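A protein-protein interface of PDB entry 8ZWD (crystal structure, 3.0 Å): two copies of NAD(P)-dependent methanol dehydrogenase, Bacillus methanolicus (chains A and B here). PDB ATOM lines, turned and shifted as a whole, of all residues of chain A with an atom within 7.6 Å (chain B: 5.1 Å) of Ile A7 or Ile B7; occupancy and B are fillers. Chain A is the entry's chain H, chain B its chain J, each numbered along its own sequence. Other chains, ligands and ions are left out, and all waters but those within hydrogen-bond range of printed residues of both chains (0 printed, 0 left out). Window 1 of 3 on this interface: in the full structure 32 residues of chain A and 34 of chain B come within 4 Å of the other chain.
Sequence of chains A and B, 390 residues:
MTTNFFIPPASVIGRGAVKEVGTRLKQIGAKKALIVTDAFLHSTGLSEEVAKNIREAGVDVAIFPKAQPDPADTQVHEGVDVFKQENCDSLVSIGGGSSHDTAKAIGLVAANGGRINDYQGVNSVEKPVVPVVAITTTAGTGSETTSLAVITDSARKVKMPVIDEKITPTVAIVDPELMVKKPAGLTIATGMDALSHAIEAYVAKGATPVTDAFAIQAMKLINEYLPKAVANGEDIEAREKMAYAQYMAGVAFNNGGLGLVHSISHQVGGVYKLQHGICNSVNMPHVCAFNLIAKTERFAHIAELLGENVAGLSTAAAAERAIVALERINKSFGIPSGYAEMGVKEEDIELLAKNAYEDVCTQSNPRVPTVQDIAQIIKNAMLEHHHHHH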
ATOM      1  N   ASN A   4       1.705   5.604 -15.538  1.00  0.00           N
ATOM      2  CA  ASN A   4       2.619   6.607 -15.010  1.00  0.00           C
ATOM      3  C   ASN A   4       2.244   7.974 -15.570  1.00  0.00           C
ATOM      4  O   ASN A   4       2.001   8.114 -16.775  1.00  0.00           O
ATOM      5  CB  ASN A   4       4.070   6.259 -15.347  1.00  0.00           C
ATOM      6  CG  ASN A   4       4.580   5.057 -14.563  1.00  0.00           C
ATOM      7  OD1 ASN A   4       3.863   4.075 -14.366  1.00  0.00           O
ATOM      8  ND2 ASN A   4       5.823   5.139 -14.099  1.00  0.00           N
ATOM      9  N   PHE A   5       2.186   8.969 -14.689  1.00  0.00           N
ATOM     10  CA  PHE A   5       1.753  10.317 -15.035  1.00  0.00           C
ATOM     11  C   PHE A   5       2.928  11.264 -14.834  1.00  0.00           C
ATOM     12  O   PHE A   5       3.336  11.518 -13.695  1.00  0.00           O
ATOM     13  CB  PHE A   5       0.553  10.728 -14.183  1.00  0.00           C
ATOM     14  CG  PHE A   5      -0.092  12.001 -14.618  1.00  0.00           C
ATOM     15  CD1 PHE A   5      -0.822  12.052 -15.790  1.00  0.00           C
ATOM     16  CD2 PHE A   5       0.024  13.146 -13.853  1.00  0.00           C
ATOM     17  CE1 PHE A   5      -1.420  13.224 -16.196  1.00  0.00           C
ATOM     18  CE2 PHE A   5      -0.577  14.325 -14.254  1.00  0.00           C
ATOM     19  CZ  PHE A   5      -1.300  14.362 -15.427  1.00  0.00           C
ATOM     20  N   PHE A   6       3.464  11.791 -15.935  1.00  0.00           N
ATOM     21  CA  PHE A   6       4.652  12.634 -15.910  1.00  0.00           C
ATOM     22  C   PHE A   6       4.285  14.051 -16.320  1.00  0.00           C
ATOM     23  O   PHE A   6       3.651  14.257 -17.356  1.00  0.00           O
ATOM     24  CB  PHE A   6       5.733  12.065 -16.829  1.00  0.00           C
ATOM     25  CG  PHE A   6       6.254  10.732 -16.378  1.00  0.00           C
ATOM     26  CD1 PHE A   6       6.303  10.423 -15.026  1.00  0.00           C
ATOM     27  CD2 PHE A   6       6.673   9.782 -17.294  1.00  0.00           C
ATOM     28  CE1 PHE A   6       6.772   9.199 -14.592  1.00  0.00           C
ATOM     29  CE2 PHE A   6       7.142   8.549 -16.866  1.00  0.00           C
ATOM     30  CZ  PHE A   6       7.193   8.260 -15.512  1.00  0.00           C
ATOM     31  N   ILE A   7       4.680  15.022 -15.507  1.00  0.00           N
ATOM     32  CA  ILE A   7       4.268  16.409 -15.704  1.00  0.00           C
ATOM     33  C   ILE A   7       5.324  17.314 -15.073  1.00  0.00           C
ATOM     34  O   ILE A   7       5.921  16.940 -14.052  1.00  0.00           O
ATOM     35  CB  ILE A   7       2.872  16.652 -15.097  1.00  0.00           C
ATOM     36  CG1 ILE A   7       2.496  18.126 -15.141  1.00  0.00           C
ATOM     37  CG2 ILE A   7       2.783  16.066 -13.677  1.00  0.00           C
ATOM     38  CD1 ILE A   7       1.014  18.401 -15.017  1.00  0.00           C
ATOM     39  N   PRO A   8       5.615  18.485 -15.641  1.00  0.00           N
ATOM     40  CA  PRO A   8       6.497  19.452 -14.956  1.00  0.00           C
ATOM     41  C   PRO A   8       6.029  19.708 -13.536  1.00  0.00           C
ATOM     42  O   PRO A   8       4.872  20.103 -13.325  1.00  0.00           O
ATOM     43  CB  PRO A   8       6.369  20.719 -15.815  1.00  0.00           C
ATOM     44  CG  PRO A   8       6.085  20.209 -17.171  1.00  0.00           C
ATOM     45  CD  PRO A   8       5.282  18.936 -17.002  1.00  0.00           C
ATOM     46  N   PRO A   9       6.889  19.489 -12.535  1.00  0.00           N
ATOM     47  CA  PRO A   9       6.453  19.685 -11.141  1.00  0.00           C
ATOM     48  C   PRO A   9       6.088  21.124 -10.806  1.00  0.00           C
ATOM     49  O   PRO A   9       5.336  21.344  -9.847  1.00  0.00           O
ATOM     50  CB  PRO A   9       7.659  19.201 -10.324  1.00  0.00           C
ATOM     51  CG  PRO A   9       8.811  19.316 -11.252  1.00  0.00           C
ATOM     52  CD  PRO A   9       8.280  19.009 -12.613  1.00  0.00           C
ATOM     53  N   ALA A  10       6.582  22.104 -11.569  1.00  0.00           N
ATOM     54  CA  ALA A  10       6.269  23.514 -11.363  1.00  0.00           C
ATOM     55  C   ALA A  10       5.880  24.142 -12.694  1.00  0.00           C
ATOM     56  O   ALA A  10       6.656  24.101 -13.655  1.00  0.00           O
ATOM     57  CB  ALA A  10       7.456  24.264 -10.750  1.00  0.00           C
ATOM     58  N   SER A  11       4.687  24.729 -12.744  1.00  0.00           N
ATOM     59  CA  SER A  11       4.185  25.395 -13.937  1.00  0.00           C
ATOM     60  C   SER A  11       3.684  26.776 -13.549  1.00  0.00           C
ATOM     61  O   SER A  11       2.953  26.916 -12.564  1.00  0.00           O
ATOM     62  CB  SER A  11       3.059  24.580 -14.595  1.00  0.00           C
ATOM     63  OG  SER A  11       3.418  23.211 -14.733  1.00  0.00           O
ATOM     64  N   GLU A 144       6.355  22.234 -23.589  1.00  0.00           N
ATOM     65  CA  GLU A 144       6.765  22.601 -22.272  1.00  0.00           C
ATOM     66  C   GLU A 144       6.350  21.562 -21.248  1.00  0.00           C
ATOM     67  O   GLU A 144       6.726  21.690 -20.098  1.00  0.00           O
ATOM     68  CB  GLU A 144       6.183  23.971 -21.949  1.00  0.00           C
ATOM     69  CG  GLU A 144       4.692  24.020 -21.669  1.00  0.00           C
ATOM     70  CD  GLU A 144       3.856  24.291 -22.896  1.00  0.00           C
ATOM     71  OE1 GLU A 144       4.419  24.335 -24.004  1.00  0.00           O
ATOM     72  OE2 GLU A 144       2.631  24.458 -22.752  1.00  0.00           O
ATOM     73  N   THR A 145       5.584  20.537 -21.642  1.00  0.00           N
ATOM     74  CA  THR A 145       5.071  19.557 -20.690  1.00  0.00           C
ATOM     75  C   THR A 145       5.238  18.116 -21.158  1.00  0.00           C
ATOM     76  O   THR A 145       4.775  17.199 -20.471  1.00  0.00           O
ATOM     77  CB  THR A 145       3.589  19.817 -20.393  1.00  0.00           C
ATOM     78  OG1 THR A 145       2.837  19.760 -21.613  1.00  0.00           O
ATOM     79  CG2 THR A 145       3.401  21.177 -19.764  1.00  0.00           C
ATOM     80  N   THR A 146       5.878  17.880 -22.293  1.00  0.00           N
ATOM     81  CA  THR A 146       5.935  16.537 -22.849  1.00  0.00           C
ATOM     82  C   THR A 146       7.285  15.892 -22.579  1.00  0.00           C
ATOM     83  O   THR A 146       8.298  16.574 -22.400  1.00  0.00           O
ATOM     84  CB  THR A 146       5.674  16.556 -24.353  1.00  0.00           C
ATOM     85  OG1 THR A 146       6.760  17.213 -25.016  1.00  0.00           O
ATOM     86  CG2 THR A 146       4.400  17.302 -24.639  1.00  0.00           C
ATOM     87  N   SER A 147       7.283  14.561 -22.545  1.00  0.00           N
ATOM     88  CA  SER A 147       8.504  13.774 -22.482  1.00  0.00           C
ATOM     89  C   SER A 147       9.012  13.408 -23.867  1.00  0.00           C
ATOM     90  O   SER A 147       9.728  12.412 -24.011  1.00  0.00           O
ATOM     91  CB  SER A 147       8.274  12.502 -21.662  1.00  0.00           C
ATOM     92  OG  SER A 147       7.648  12.783 -20.425  1.00  0.00           O
ATOM     93  N   GLU A 165      11.299   9.814 -19.932  1.00  0.00           N
ATOM     94  CA  GLU A 165      10.746  10.587 -18.820  1.00  0.00           C
ATOM     95  C   GLU A 165      11.737  11.612 -18.289  1.00  0.00           C
ATOM     96  O   GLU A 165      11.326  12.634 -17.732  1.00  0.00           O
ATOM     97  CB  GLU A 165      10.301   9.664 -17.681  1.00  0.00           C
ATOM     98  CG  GLU A 165      11.333   8.652 -17.218  1.00  0.00           C
ATOM     99  CD  GLU A 165      10.820   7.788 -16.078  1.00  0.00           C
ATOM    100  OE1 GLU A 165      10.516   8.344 -15.003  1.00  0.00           O
ATOM    101  OE2 GLU A 165      10.710   6.555 -16.261  1.00  0.00           O
ATOM    102  N   THR A 168      11.263  15.248 -19.582  1.00  0.00           N
ATOM    103  CA  THR A 168      10.114  16.061 -19.206  1.00  0.00           C
ATOM    104  C   THR A 168      10.638  17.345 -18.584  1.00  0.00           C
ATOM    105  O   THR A 168      11.442  17.278 -17.641  1.00  0.00           O
ATOM    106  CB  THR A 168       9.215  15.335 -18.214  1.00  0.00           C
ATOM    107  OG1 THR A 168       9.038  13.974 -18.629  1.00  0.00           O
ATOM    108  CG2 THR A 168       7.853  16.007 -18.142  1.00  0.00           C
ATOM    109  N   PRO A 169      10.243  18.519 -19.077  1.00  0.00           N
ATOM    110  CA  PRO A 169      10.817  19.759 -18.544  1.00  0.00           C
ATOM    111  C   PRO A 169      10.560  19.878 -17.051  1.00  0.00           C
ATOM    112  O   PRO A 169       9.551  19.402 -16.530  1.00  0.00           O
ATOM    113  CB  PRO A 169      10.089  20.855 -19.328  1.00  0.00           C
ATOM    114  CG  PRO A 169       9.668  20.193 -20.591  1.00  0.00           C
ATOM    115  CD  PRO A 169       9.340  18.771 -20.214  1.00  0.00           C
ATOM    116  N   THR A 170      11.509  20.498 -16.354  1.00  0.00           N
ATOM    117  CA  THR A 170      11.375  20.646 -14.911  1.00  0.00           C
ATOM    118  C   THR A 170      10.456  21.805 -14.561  1.00  0.00           C
ATOM    119  O   THR A 170       9.641  21.691 -13.639  1.00  0.00           O
ATOM    120  CB  THR A 170      12.747  20.835 -14.255  1.00  0.00           C
ATOM    121  OG1 THR A 170      13.644  19.821 -14.736  1.00  0.00           O
ATOM    122  CG2 THR A 170      12.627  20.725 -12.740  1.00  0.00           C
ATOM    123  N   ALA A 172       7.726  24.705 -16.335  1.00  0.00           N
ATOM    124  CA  ALA A 172       7.008  25.193 -17.503  1.00  0.00           C
ATOM    125  C   ALA A 172       6.575  26.637 -17.294  1.00  0.00           C
ATOM    126  O   ALA A 172       6.099  27.000 -16.216  1.00  0.00           O
ATOM    127  CB  ALA A 172       5.776  24.330 -17.794  1.00  0.00           C
ATOM    128  N   VAL A 210      -7.542  10.869 -15.729  1.00  0.00           N
ATOM    129  CA  VAL A 210      -6.763  12.085 -15.517  1.00  0.00           C
ATOM    130  C   VAL A 210      -6.515  12.804 -16.838  1.00  0.00           C
ATOM    131  O   VAL A 210      -6.827  13.993 -16.978  1.00  0.00           O
ATOM    132  CB  VAL A 210      -5.446  11.757 -14.792  1.00  0.00           C
ATOM    133  CG1 VAL A 210      -4.582  13.003 -14.660  1.00  0.00           C
ATOM    134  CG2 VAL A 210      -5.737  11.174 -13.424  1.00  0.00           C
ATOM    135  N   PHE A 214      -8.156  16.803 -18.692  1.00  0.00           N
ATOM    136  CA  PHE A 214      -7.447  17.848 -19.411  1.00  0.00           C
ATOM    137  C   PHE A 214      -7.896  17.915 -20.864  1.00  0.00           C
ATOM    138  O   PHE A 214      -8.048  19.005 -21.418  1.00  0.00           O
ATOM    139  CB  PHE A 214      -5.938  17.622 -19.309  1.00  0.00           C
ATOM    140  CG  PHE A 214      -5.309  18.222 -18.074  1.00  0.00           C
ATOM    141  CD1 PHE A 214      -6.052  18.989 -17.191  1.00  0.00           C
ATOM    142  CD2 PHE A 214      -3.962  18.029 -17.809  1.00  0.00           C
ATOM    143  CE1 PHE A 214      -5.454  19.545 -16.058  1.00  0.00           C
ATOM    144  CE2 PHE A 214      -3.364  18.580 -16.686  1.00  0.00           C
ATOM    145  CZ  PHE A 214      -4.104  19.336 -15.810  1.00  0.00           C
ATOM    146  N   TYR A 247      -1.588  23.835 -22.739  1.00  0.00           N
ATOM    147  CA  TYR A 247      -0.938  23.159 -21.621  1.00  0.00           C
ATOM    148  C   TYR A 247      -1.654  21.855 -21.293  1.00  0.00           C
ATOM    149  O   TYR A 247      -1.031  20.783 -21.210  1.00  0.00           O
ATOM    150  CB  TYR A 247      -0.902  24.092 -20.407  1.00  0.00           C
ATOM    151  CG  TYR A 247      -0.360  23.489 -19.131  1.00  0.00           C
ATOM    152  CD1 TYR A 247      -1.208  22.870 -18.220  1.00  0.00           C
ATOM    153  CD2 TYR A 247       0.991  23.560 -18.822  1.00  0.00           C
ATOM    154  CE1 TYR A 247      -0.723  22.320 -17.052  1.00  0.00           C
ATOM    155  CE2 TYR A 247       1.485  23.017 -17.649  1.00  0.00           C
ATOM    156  CZ  TYR A 247       0.623  22.395 -16.770  1.00  0.00           C
ATOM    157  OH  TYR A 247       1.108  21.852 -15.603  1.00  0.00           O
ATOM    158  N   VAL A 251      -0.217  17.898 -21.625  1.00  0.00           N
ATOM    159  CA  VAL A 251      -0.217  16.885 -20.569  1.00  0.00           C
ATOM    160  C   VAL A 251      -0.992  15.654 -21.027  1.00  0.00           C
ATOM    161  O   VAL A 251      -0.513  14.509 -20.933  1.00  0.00           O
ATOM    162  CB  VAL A 251      -0.806  17.462 -19.271  1.00  0.00           C
ATOM    163  CG1 VAL A 251      -0.683  16.452 -18.148  1.00  0.00           C
ATOM    164  CG2 VAL A 251      -0.120  18.764 -18.907  1.00  0.00           C
ATOM    165  N   ASN A 254       0.840  13.684 -23.749  1.00  0.00           N
ATOM    166  CA  ASN A 254       2.060  13.061 -23.267  1.00  0.00           C
ATOM    167  C   ASN A 254       1.733  11.769 -22.548  1.00  0.00           C
ATOM    168  O   ASN A 254       2.377  10.739 -22.773  1.00  0.00           O
ATOM    169  CB  ASN A 254       2.813  14.014 -22.348  1.00  0.00           C
ATOM    170  CG  ASN A 254       4.241  13.585 -22.128  1.00  0.00           C
ATOM    171  OD1 ASN A 254       4.926  13.177 -23.066  1.00  0.00           O
ATOM    172  ND2 ASN A 254       4.699  13.665 -20.889  1.00  0.00           N
ATOM    173  N   ASN A 255       0.705  11.792 -21.704  1.00  0.00           N
ATOM    174  CA  ASN A 255       0.444  10.572 -20.947  1.00  0.00           C
ATOM    175  C   ASN A 255      -0.535   9.624 -21.636  1.00  0.00           C
ATOM    176  O   ASN A 255      -0.376   8.406 -21.544  1.00  0.00           O
ATOM    177  CB  ASN A 255      -0.057  10.930 -19.547  1.00  0.00           C
ATOM    178  CG  ASN A 255       0.983  11.709 -18.761  1.00  0.00           C
ATOM    179  OD1 ASN A 255       1.888  11.128 -18.162  1.00  0.00           O
ATOM    180  ND2 ASN A 255       0.873  13.033 -18.781  1.00  0.00           N
ATOM    181  N   PHE B   5       1.258  26.164 -10.587  1.00  0.00           N
ATOM    182  CA  PHE B   5       0.647  24.839 -10.514  1.00  0.00           C
ATOM    183  C   PHE B   5       1.720  23.848 -10.080  1.00  0.00           C
ATOM    184  O   PHE B   5       2.655  23.565 -10.837  1.00  0.00           O
ATOM    185  CB  PHE B   5       0.028  24.434 -11.855  1.00  0.00           C
ATOM    186  CG  PHE B   5      -0.762  23.158 -11.801  1.00  0.00           C
ATOM    187  CD1 PHE B   5      -2.021  23.132 -11.223  1.00  0.00           C
ATOM    188  CD2 PHE B   5      -0.248  21.982 -12.336  1.00  0.00           C
ATOM    189  CE1 PHE B   5      -2.749  21.954 -11.168  1.00  0.00           C
ATOM    190  CE2 PHE B   5      -0.978  20.796 -12.288  1.00  0.00           C
ATOM    191  CZ  PHE B   5      -2.228  20.784 -11.707  1.00  0.00           C
ATOM    192  N   PHE B   6       1.588  23.328  -8.862  1.00  0.00           N
ATOM    193  CA  PHE B   6       2.571  22.429  -8.276  1.00  0.00           C
ATOM    194  C   PHE B   6       1.963  21.043  -8.128  1.00  0.00           C
ATOM    195  O   PHE B   6       0.936  20.872  -7.464  1.00  0.00           O
ATOM    196  CB  PHE B   6       3.056  22.965  -6.929  1.00  0.00           C
ATOM    197  CG  PHE B   6       3.735  24.299  -7.023  1.00  0.00           C
ATOM    198  CD1 PHE B   6       4.508  24.617  -8.133  1.00  0.00           C
ATOM    199  CD2 PHE B   6       3.591  25.243  -6.018  1.00  0.00           C
ATOM    200  CE1 PHE B   6       5.136  25.848  -8.231  1.00  0.00           C
ATOM    201  CE2 PHE B   6       4.214  26.478  -6.112  1.00  0.00           C
ATOM    202  CZ  PHE B   6       4.987  26.779  -7.219  1.00  0.00           C
ATOM    203  N   ILE B   7       2.609  20.061  -8.750  1.00  0.00           N
ATOM    204  CA  ILE B   7       2.125  18.683  -8.765  1.00  0.00           C
ATOM    205  C   ILE B   7       3.317  17.751  -8.666  1.00  0.00           C
ATOM    206  O   ILE B   7       4.419  18.075  -9.130  1.00  0.00           O
ATOM    207  CB  ILE B   7       1.320  18.388 -10.058  1.00  0.00           C
ATOM    208  CG1 ILE B   7       0.678  16.999 -10.048  1.00  0.00           C
ATOM    209  CG2 ILE B   7       2.195  18.604 -11.290  1.00  0.00           C
ATOM    210  CD1 ILE B   7      -0.547  16.908 -10.932  1.00  0.00           C
ATOM    211  N   PRO B   8       3.150  16.617  -7.985  1.00  0.00           N
ATOM    212  CA  PRO B   8       4.204  15.596  -7.978  1.00  0.00           C
ATOM    213  C   PRO B   8       4.688  15.307  -9.386  1.00  0.00           C
ATOM    214  O   PRO B   8       3.878  15.111 -10.305  1.00  0.00           O
ATOM    215  CB  PRO B   8       3.505  14.376  -7.360  1.00  0.00           C
ATOM    216  CG  PRO B   8       2.517  14.977  -6.431  1.00  0.00           C
ATOM    217  CD  PRO B   8       2.070  16.291  -7.034  1.00  0.00           C
ATOM    218  N   PRO B   9       6.002  15.306  -9.605  1.00  0.00           N
ATOM    219  CA  PRO B   9       6.513  15.074 -10.965  1.00  0.00           C
ATOM    220  C   PRO B   9       6.191  13.693 -11.509  1.00  0.00           C
ATOM    221  O   PRO B   9       6.110  13.527 -12.733  1.00  0.00           O
ATOM    222  CB  PRO B   9       8.025  15.282 -10.807  1.00  0.00           C
ATOM    223  CG  PRO B   9       8.293  15.023  -9.352  1.00  0.00           C
ATOM    224  CD  PRO B   9       7.084  15.545  -8.635  1.00  0.00           C
ATOM    225  N   THR B 168       5.823  19.430  -1.512  1.00  0.00           N
ATOM    226  CA  THR B 168       5.047  18.718  -2.516  1.00  0.00           C
ATOM    227  C   THR B 168       5.735  17.387  -2.793  1.00  0.00           C
ATOM    228  O   THR B 168       6.950  17.361  -3.027  1.00  0.00           O
ATOM    229  CB  THR B 168       4.913  19.531  -3.799  1.00  0.00           C
ATOM    230  OG1 THR B 168       4.448  20.847  -3.483  1.00  0.00           O
ATOM    231  CG2 THR B 168       3.914  18.868  -4.721  1.00  0.00           C
ATOM    232  N   PRO B 169       5.015  16.269  -2.732  1.00  0.00           N
ATOM    233  CA  PRO B 169       5.676  14.965  -2.807  1.00  0.00           C
ATOM    234  C   PRO B 169       6.345  14.736  -4.150  1.00  0.00           C
ATOM    235  O   PRO B 169       5.873  15.187  -5.197  1.00  0.00           O
ATOM    236  CB  PRO B 169       4.527  13.973  -2.579  1.00  0.00           C
ATOM    237  CG  PRO B 169       3.506  14.758  -1.846  1.00  0.00           C
ATOM    238  CD  PRO B 169       3.584  16.132  -2.434  1.00  0.00           C
ATOM    239  N   PHE B 214      -9.749  19.098 -13.251  1.00  0.00           N
ATOM    240  CA  PHE B 214      -9.688  17.997 -12.301  1.00  0.00           C
ATOM    241  C   PHE B 214     -10.893  18.005 -11.369  1.00  0.00           C
ATOM    242  O   PHE B 214     -11.427  16.940 -11.029  1.00  0.00           O
ATOM    243  CB  PHE B 214      -8.386  18.067 -11.501  1.00  0.00           C
ATOM    244  CG  PHE B 214      -7.194  17.533 -12.235  1.00  0.00           C
ATOM    245  CD1 PHE B 214      -7.310  17.026 -13.520  1.00  0.00           C
ATOM    246  CD2 PHE B 214      -5.953  17.525 -11.628  1.00  0.00           C
ATOM    247  CE1 PHE B 214      -6.202  16.533 -14.187  1.00  0.00           C
ATOM    248  CE2 PHE B 214      -4.852  17.034 -12.285  1.00  0.00           C
ATOM    249  CZ  PHE B 214      -4.971  16.540 -13.562  1.00  0.00           C
ATOM    250  N   TYR B 247      -7.099  11.778  -6.284  1.00  0.00           N
ATOM    251  CA  TYR B 247      -5.889  12.407  -6.811  1.00  0.00           C
ATOM    252  C   TYR B 247      -6.223  13.742  -7.473  1.00  0.00           C
ATOM    253  O   TYR B 247      -5.620  14.784  -7.160  1.00  0.00           O
ATOM    254  CB  TYR B 247      -5.198  11.454  -7.794  1.00  0.00           C
ATOM    255  CG  TYR B 247      -3.924  11.983  -8.432  1.00  0.00           C
ATOM    256  CD1 TYR B 247      -3.974  12.798  -9.559  1.00  0.00           C
ATOM    257  CD2 TYR B 247      -2.674  11.645  -7.923  1.00  0.00           C
ATOM    258  CE1 TYR B 247      -2.816  13.280 -10.152  1.00  0.00           C
ATOM    259  CE2 TYR B 247      -1.505  12.119  -8.515  1.00  0.00           C
ATOM    260  CZ  TYR B 247      -1.582  12.941  -9.626  1.00  0.00           C
ATOM    261  OH  TYR B 247      -0.423  13.416 -10.210  1.00  0.00           O
ATOM    262  N   VAL B 251      -5.042  17.603  -6.085  1.00  0.00           N
ATOM    263  CA  VAL B 251      -4.272  18.557  -6.885  1.00  0.00           C
ATOM    264  C   VAL B 251      -5.083  19.830  -7.132  1.00  0.00           C
ATOM    265  O   VAL B 251      -4.547  20.955  -7.103  1.00  0.00           O
ATOM    266  CB  VAL B 251      -3.828  17.907  -8.207  1.00  0.00           C
ATOM    267  CG1 VAL B 251      -2.976  18.866  -9.007  1.00  0.00           C
ATOM    268  CG2 VAL B 251      -3.067  16.631  -7.942  1.00  0.00           C
ATOM    269  N   ASN B 255      -3.819  23.676  -5.717  1.00  0.00           N
ATOM    270  CA  ASN B 255      -3.439  24.773  -6.588  1.00  0.00           C
ATOM    271  C   ASN B 255      -4.589  25.710  -6.918  1.00  0.00           C
ATOM    272  O   ASN B 255      -4.507  26.498  -7.846  1.00  0.00           O
ATOM    273  CB  ASN B 255      -2.760  24.232  -7.834  1.00  0.00           C
ATOM    274  CG  ASN B 255      -1.581  23.362  -7.510  1.00  0.00           C
ATOM    275  OD1 ASN B 255      -0.543  23.852  -7.092  1.00  0.00           O
ATOM    276  ND2 ASN B 255      -1.739  22.061  -7.682  1.00  0.00           N
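O of Pro B9 touches O of Phe A5 (3.6 Å).
OH of Tyr B247 touches CD2 of Phe A5 (3.7 Å).
CA of Phe A6 touches O of Pro B9, 3.6 Å away.
CG2 of Ile A7 touches CG2 of Ile B7, at 3.5 Å.
Ile A7 touches Pro B8.
Pro A9 touches Phe B5 (O to O, 3.6 Å).
Pro B9 touches Pro A9 (CB to CB, 3.97 Å).
Phe B6 touches Ala A10.
Phe B214 touches Val A210.
CE1 of Phe A214 touches CE1 of Phe B214, 3.6 Å away.
Asn A254 touches none of the printed residues of chain B.
Ile B7 touches just these residues of chain A: Ile A7, Pro A8 and Pro A9.
Printed residues of chain A within 4 Å of Pro B8: Ile A7 (3.7 Å).
Of the printed residues of chain A, Pro B9 touches Phe A5, Phe A6, Ile A7 and Pro A9.
Printed residues of chain A within 4 Å of Phe B214: Val A210 (3.7 Å) and Phe A214 (3.6 Å).
The nearest residue of chain B that does not touch Ile A7 is Phe B5 (4.1 Å).
The nearest residue of chain A that does not touch Ile B7 is Phe A5 (4.2 Å).
The nearest printed residue of chain B that does not touch Val A210 is Tyr B247 (4.5 Å).
N of Phe B6 is in hydrogen-bond range of OD1 of Asn B255 (2.8 Å).
The side-chain amide oxygen (OD1) of Asn A255 is in hydrogen-bond range of the backbone NH (N) of Phe A6, at 2.8 Å.
The backbone carbonyl oxygen of Ala A10 is in hydrogen-bond range of the backbone NH of Ala A172 (2.9 Å).
The side-chain hydroxyl (OH) of Tyr A247 lies within hydrogen-bond range of the side-chain hydroxyl (OG) of Ser A11, at 2.8 Å.
Phe A6 touches Pro B9, and with the chains exchanged Pro A9 touches Phe B6.
Ile B7 touches its own counterpart, Ile A7.
Ile A7 touches Pro B9, and with the chains exchanged Pro A9 touches Ile B7.
Pro A9 touches its own counterpart, Pro B9.
The backbone NH (N) of Ile A7 sits at hydrogen-bond distance from the backbone carbonyl oxygen (O) of Pro B9.
The backbone carbonyl oxygen (O) of Pro A9 is in hydrogen-bond range of the backbone NH (N) of Ile B7 (3.2 Å).
The backbone carbonyl oxygen (O) of Ser A11 lies within hydrogen-bond range of the backbone NH (N) of Phe B5 (2.7 Å).
Hydrophobic or aromatic side chains of chain A within 4 Å of the printed part of chain B: Phe A5, Phe A6, Ile A7, Pro A9, Ala A10, Val A210, Phe A214 and Tyr A247.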
